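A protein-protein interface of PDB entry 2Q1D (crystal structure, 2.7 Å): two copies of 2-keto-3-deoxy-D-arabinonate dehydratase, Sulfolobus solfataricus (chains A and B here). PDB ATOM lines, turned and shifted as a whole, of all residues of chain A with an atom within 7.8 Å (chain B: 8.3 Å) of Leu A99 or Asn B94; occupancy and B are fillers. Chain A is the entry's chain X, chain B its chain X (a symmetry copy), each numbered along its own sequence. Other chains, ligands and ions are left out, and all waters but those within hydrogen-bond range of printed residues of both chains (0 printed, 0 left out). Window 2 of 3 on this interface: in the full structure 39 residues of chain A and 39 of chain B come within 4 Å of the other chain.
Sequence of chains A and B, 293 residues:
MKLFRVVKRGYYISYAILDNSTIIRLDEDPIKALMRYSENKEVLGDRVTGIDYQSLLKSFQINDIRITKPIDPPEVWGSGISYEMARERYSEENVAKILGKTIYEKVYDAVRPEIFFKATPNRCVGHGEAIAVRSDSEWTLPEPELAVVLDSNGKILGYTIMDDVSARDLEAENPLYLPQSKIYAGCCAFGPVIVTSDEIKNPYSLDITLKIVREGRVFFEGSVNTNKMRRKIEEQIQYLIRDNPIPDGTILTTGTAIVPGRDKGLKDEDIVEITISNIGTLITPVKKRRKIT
Ala A96 touches Lys B97, and with the chains exchanged Lys A97 touches Ala B96.
Lys B97 touches its own counterpart, Lys A97.
Positions printed for both chains: 96, 97 and 102.
Of the 10 pairs that touch across the chains among the printed residues, 3 have their exchanged pair printed and touching as well.
Leu A99 touches just one residue of chain B: Asn B94 (3.1 Å).
Of the printed residues of chain B, Lys A97 touches Val B95, Ala B96 and Lys B97.
Of the printed residues of chain B, Lys A106 touches Glu B173 (3.4 Å) and Asn B174 (3.9 Å).
Ala B172 touches none of the printed residues of chain A.
Lys A101 touches none of the printed residues of chain B.
The nearest residue of chain B that does not touch Leu A99 is Val B95 (5.1 Å).
The nearest printed residue of chain A that does not touch Lys B97 is Ile A98 (5.2 Å).
Among the printed residues, merely in contact across the chains: Leu A99 with Asn B94, Ile A98 with Ala B96, Lys A97 with Ala B96, Ala A96 with Lys B97, Ile A98 with Val B95, Ile A98 with Asn B94, Lys A106 with Asn B174 and Lys A97 with Val B95.
N of Lys A97 sits at hydrogen-bond distance from O of Lys B97 (3.2 Å).
The backbone carbonyl oxygen of Glu B173 is in hydrogen-bond range of the side-chain amino group of Lys A106, at 3.4 Å.
Of the 9 printed residues of chain B, 6 touch a printed residue of chain A.
Along chain B the printed residues that touch a printed residue of chain A span positions 94 to 174.
Of the 9 printed residues of chain A, 5 touch a printed residue of chain B.
Along chain A the printed residues that touch a printed residue of chain B span positions 96 to 106.
Among the printed residues, 10 pairs touch across the chains.
Among the printed residues, no Asp or Glu carboxylate lies within 4 Å of a Lys or Arg side-chain nitrogen of the other chain.
The backbone carbonyl oxygen of Ala A96 sits at hydrogen-bond distance from the side-chain hydroxyl of Thr A102 (3.3 Å).
The backbone carbonyl oxygen of Ala B96 is in hydrogen-bond range of the side-chain hydroxyl of Thr B102 (3.3 Å).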
ATOM      1  N   ALA A  96     -10.320  -1.942  19.238  1.00  0.00           N
ATOM      2  CA  ALA A  96     -10.638  -1.031  20.337  1.00  0.00           C
ATOM      3  C   ALA A  96     -12.064  -1.191  20.828  1.00  0.00           C
ATOM      4  O   ALA A  96     -13.004  -1.225  20.035  1.00  0.00           O
ATOM      5  CB  ALA A  96     -10.393   0.401  19.912  1.00  0.00           C
ATOM      6  N   LYS A  97     -12.222  -1.269  22.143  1.00  0.00           N
ATOM      7  CA  LYS A  97     -13.550  -1.411  22.731  1.00  0.00           C
ATOM      8  C   LYS A  97     -13.767  -0.538  23.974  1.00  0.00           C
ATOM      9  O   LYS A  97     -12.846  -0.337  24.766  1.00  0.00           O
ATOM     10  CB  LYS A  97     -13.882  -2.895  22.985  1.00  0.00           C
ATOM     11  CG  LYS A  97     -12.697  -3.778  23.423  1.00  0.00           C
ATOM     12  CD  LYS A  97     -12.711  -5.166  22.750  1.00  0.00           C
ATOM     13  CE  LYS A  97     -13.874  -6.047  23.222  1.00  0.00           C
ATOM     14  NZ  LYS A  97     -13.854  -7.405  22.604  1.00  0.00           N
ATOM     15  N   ILE A  98     -14.977   0.016  24.087  1.00  0.00           N
ATOM     16  CA  ILE A  98     -15.441   0.743  25.275  1.00  0.00           C
ATOM     17  C   ILE A  98     -16.397  -0.178  26.007  1.00  0.00           C
ATOM     18  O   ILE A  98     -17.480  -0.491  25.484  1.00  0.00           O
ATOM     19  CB  ILE A  98     -16.265   2.024  24.932  1.00  0.00           C
ATOM     20  CG1 ILE A  98     -15.618   2.855  23.812  1.00  0.00           C
ATOM     21  CG2 ILE A  98     -16.558   2.844  26.211  1.00  0.00           C
ATOM     22  CD1 ILE A  98     -14.690   3.954  24.288  1.00  0.00           C
ATOM     23  N   LEU A  99     -16.009  -0.594  27.215  1.00  0.00           N
ATOM     24  CA  LEU A  99     -16.799  -1.541  28.023  1.00  0.00           C
ATOM     25  C   LEU A  99     -17.197  -2.802  27.227  1.00  0.00           C
ATOM     26  O   LEU A  99     -18.389  -3.102  27.082  1.00  0.00           O
ATOM     27  CB  LEU A  99     -18.058  -0.867  28.608  1.00  0.00           C
ATOM     28  CG  LEU A  99     -18.027   0.603  29.052  1.00  0.00           C
ATOM     29  CD1 LEU A  99     -19.444   1.119  29.371  1.00  0.00           C
ATOM     30  CD2 LEU A  99     -17.059   0.821  30.220  1.00  0.00           C
ATOM     31  N   GLY A 100     -16.198  -3.515  26.699  1.00  0.00           N
ATOM     32  CA  GLY A 100     -16.424  -4.763  25.959  1.00  0.00           C
ATOM     33  C   GLY A 100     -17.309  -4.638  24.726  1.00  0.00           C
ATOM     34  O   GLY A 100     -17.744  -5.642  24.153  1.00  0.00           O
ATOM     35  N   LYS A 101     -17.589  -3.402  24.329  1.00  0.00           N
ATOM     36  CA  LYS A 101     -18.296  -3.121  23.089  1.00  0.00           C
ATOM     37  C   LYS A 101     -17.305  -2.453  22.126  1.00  0.00           C
ATOM     38  O   LYS A 101     -16.544  -1.568  22.531  1.00  0.00           O
ATOM     39  CB  LYS A 101     -19.496  -2.221  23.372  1.00  0.00           C
ATOM     40  CG  LYS A 101     -20.570  -2.275  22.311  1.00  0.00           C
ATOM     41  CD  LYS A 101     -21.935  -1.941  22.893  1.00  0.00           C
ATOM     42  CE  LYS A 101     -23.020  -2.042  21.828  1.00  0.00           C
ATOM     43  NZ  LYS A 101     -24.312  -2.488  22.413  1.00  0.00           N
ATOM     44  N   THR A 102     -17.293  -2.894  20.868  1.00  0.00           N
ATOM     45  CA  THR A 102     -16.300  -2.421  19.900  1.00  0.00           C
ATOM     46  C   THR A 102     -16.654  -1.015  19.408  1.00  0.00           C
ATOM     47  O   THR A 102     -17.813  -0.743  19.087  1.00  0.00           O
ATOM     48  CB  THR A 102     -16.098  -3.439  18.732  1.00  0.00           C
ATOM     49  OG1 THR A 102     -14.724  -3.444  18.338  1.00  0.00           O
ATOM     50  CG2 THR A 102     -16.969  -3.139  17.505  1.00  0.00           C
ATOM     51  N   GLU A 105     -19.097  -0.823  16.560  1.00  0.00           N
ATOM     52  CA  GLU A 105     -20.486  -1.199  16.804  1.00  0.00           C
ATOM     53  C   GLU A 105     -21.194  -0.176  17.712  1.00  0.00           C
ATOM     54  O   GLU A 105     -22.415  -0.010  17.641  1.00  0.00           O
ATOM     55  CB  GLU A 105     -20.610  -2.648  17.305  1.00  0.00           C
ATOM     56  CG  GLU A 105     -20.205  -2.884  18.748  1.00  0.00           C
ATOM     57  CD  GLU A 105     -19.802  -4.327  19.029  1.00  0.00           C
ATOM     58  OE1 GLU A 105     -20.155  -5.225  18.236  1.00  0.00           O
ATOM     59  OE2 GLU A 105     -19.116  -4.561  20.048  1.00  0.00           O
ATOM     60  N   LYS A 106     -20.407   0.525  18.528  1.00  0.00           N
ATOM     61  CA  LYS A 106     -20.898   1.644  19.340  1.00  0.00           C
ATOM     62  C   LYS A 106     -21.385   2.821  18.468  1.00  0.00           C
ATOM     63  O   LYS A 106     -22.494   3.328  18.677  1.00  0.00           O
ATOM     64  CB  LYS A 106     -19.825   2.070  20.345  1.00  0.00           C
ATOM     65  CG  LYS A 106     -20.308   3.029  21.405  1.00  0.00           C
ATOM     66  CD  LYS A 106     -19.843   2.596  22.791  1.00  0.00           C
ATOM     67  CE  LYS A 106     -19.417   3.778  23.654  1.00  0.00           C
ATOM     68  NZ  LYS A 106     -20.354   4.939  23.563  1.00  0.00           N
ATOM     69  N   ASN B  94     -12.434   4.747  31.900  1.00  0.00           N
ATOM     70  CA  ASN B  94     -13.630   4.279  31.196  1.00  0.00           C
ATOM     71  C   ASN B  94     -13.668   4.530  29.662  1.00  0.00           C
ATOM     72  O   ASN B  94     -14.736   4.558  29.026  1.00  0.00           O
ATOM     73  CB  ASN B  94     -14.873   4.863  31.848  1.00  0.00           C
ATOM     74  CG  ASN B  94     -16.090   4.021  31.585  1.00  0.00           C
ATOM     75  OD1 ASN B  94     -16.886   4.315  30.687  1.00  0.00           O
ATOM     76  ND2 ASN B  94     -16.218   2.927  32.332  1.00  0.00           N
ATOM     77  N   VAL B  95     -12.480   4.692  29.082  1.00  0.00           N
ATOM     78  CA  VAL B  95     -12.329   5.032  27.671  1.00  0.00           C
ATOM     79  C   VAL B  95     -11.986   3.807  26.831  1.00  0.00           C
ATOM     80  O   VAL B  95     -12.142   2.678  27.290  1.00  0.00           O
ATOM     81  CB  VAL B  95     -11.277   6.176  27.460  1.00  0.00           C
ATOM     82  CG1 VAL B  95     -11.908   7.567  27.735  1.00  0.00           C
ATOM     83  CG2 VAL B  95     -10.008   5.940  28.304  1.00  0.00           C
ATOM     84  N   ALA B  96     -11.521   4.043  25.606  1.00  0.00           N
ATOM     85  CA  ALA B  96     -11.225   2.983  24.643  1.00  0.00           C
ATOM     86  C   ALA B  96      -9.924   2.267  24.952  1.00  0.00           C
ATOM     87  O   ALA B  96      -8.898   2.899  25.199  1.00  0.00           O
ATOM     88  CB  ALA B  96     -11.182   3.553  23.241  1.00  0.00           C
ATOM     89  N   LYS B  97      -9.968   0.941  24.919  1.00  0.00           N
ATOM     90  CA  LYS B  97      -8.774   0.145  25.186  1.00  0.00           C
ATOM     91  C   LYS B  97      -8.602  -1.043  24.232  1.00  0.00           C
ATOM     92  O   LYS B  97      -9.584  -1.665  23.824  1.00  0.00           O
ATOM     93  CB  LYS B  97      -8.715  -0.274  26.669  1.00  0.00           C
ATOM     94  CG  LYS B  97     -10.072  -0.591  27.327  1.00  0.00           C
ATOM     95  CD  LYS B  97     -10.178  -0.040  28.764  1.00  0.00           C
ATOM     96  CE  LYS B  97      -9.244  -0.754  29.748  1.00  0.00           C
ATOM     97  NZ  LYS B  97      -9.386  -0.250  31.145  1.00  0.00           N
ATOM     98  N   THR B 102      -5.081   1.284  27.364  1.00  0.00           N
ATOM     99  CA  THR B 102      -5.841   2.428  26.856  1.00  0.00           C
ATOM    100  C   THR B 102      -5.209   2.968  25.571  1.00  0.00           C
ATOM    101  O   THR B 102      -3.987   3.127  25.499  1.00  0.00           O
ATOM    102  CB  THR B 102      -6.032   3.529  27.947  1.00  0.00           C
ATOM    103  OG1 THR B 102      -7.320   4.129  27.798  1.00  0.00           O
ATOM    104  CG2 THR B 102      -4.960   4.626  27.899  1.00  0.00           C
ATOM    105  N   ALA B 172     -14.193  11.588  24.313  1.00  0.00           N
ATOM    106  CA  ALA B 172     -14.191  10.550  25.339  1.00  0.00           C
ATOM    107  C   ALA B 172     -15.379   9.619  25.145  1.00  0.00           C
ATOM    108  O   ALA B 172     -15.353   8.459  25.571  1.00  0.00           O
ATOM    109  CB  ALA B 172     -14.212  11.171  26.725  1.00  0.00           C
ATOM    110  N   GLU B 173     -16.413  10.129  24.487  1.00  0.00           N
ATOM    111  CA  GLU B 173     -17.576   9.325  24.151  1.00  0.00           C
ATOM    112  C   GLU B 173     -17.246   8.222  23.128  1.00  0.00           C
ATOM    113  O   GLU B 173     -17.817   7.131  23.184  1.00  0.00           O
ATOM    114  CB  GLU B 173     -18.683  10.222  23.629  1.00  0.00           C
ATOM    115  CG  GLU B 173     -20.033   9.570  23.600  1.00  0.00           C
ATOM    116  CD  GLU B 173     -21.076  10.483  23.000  1.00  0.00           C
ATOM    117  OE1 GLU B 173     -21.003  11.711  23.270  1.00  0.00           O
ATOM    118  OE2 GLU B 173     -21.954   9.976  22.250  1.00  0.00           O
ATOM    119  N   ASN B 174     -16.329   8.525  22.205  1.00  0.00           N
ATOM    120  CA  ASN B 174     -15.854   7.606  21.157  1.00  0.00           C
ATOM    121  C   ASN B 174     -14.719   8.278  20.397  1.00  0.00           C
ATOM    122  O   ASN B 174     -14.878   9.408  19.946  1.00  0.00           O
ATOM    123  CB  ASN B 174     -16.977   7.258  20.172  1.00  0.00           C
ATOM    124  CG  ASN B 174     -16.698   5.991  19.383  1.00  0.00           C
ATOM    125  OD1 ASN B 174     -15.580   5.764  18.904  1.00  0.00           O
ATOM    126  ND2 ASN B 174     -17.724   5.153  19.244  1.00  0.00           N
ATOM    127  N   ARG B 262     -12.895  17.939  34.573  1.00  0.00           N
ATOM    128  CA  ARG B 262     -14.197  17.810  33.900  1.00  0.00           C
ATOM    129  C   ARG B 262     -15.209  18.902  34.233  1.00  0.00           C
ATOM    130  O   ARG B 262     -16.239  19.022  33.561  1.00  0.00           O
ATOM    131  CB  ARG B 262     -14.811  16.425  34.139  1.00  0.00           C
ATOM    132  CG  ARG B 262     -15.084  15.677  32.772  1.00  0.00           C
ATOM    133  CD  ARG B 262     -15.443  14.221  33.060  1.00  0.00           C
ATOM    134  NE  ARG B 262     -14.253  13.338  33.073  1.00  0.00           N
ATOM    135  CZ  ARG B 262     -14.126  12.252  33.844  1.00  0.00           C
ATOM    136  NH1 ARG B 262     -13.009  11.511  33.776  1.00  0.00           N
ATOM    137  NH2 ARG B 262     -15.110  11.908  34.693  1.00  0.00           N
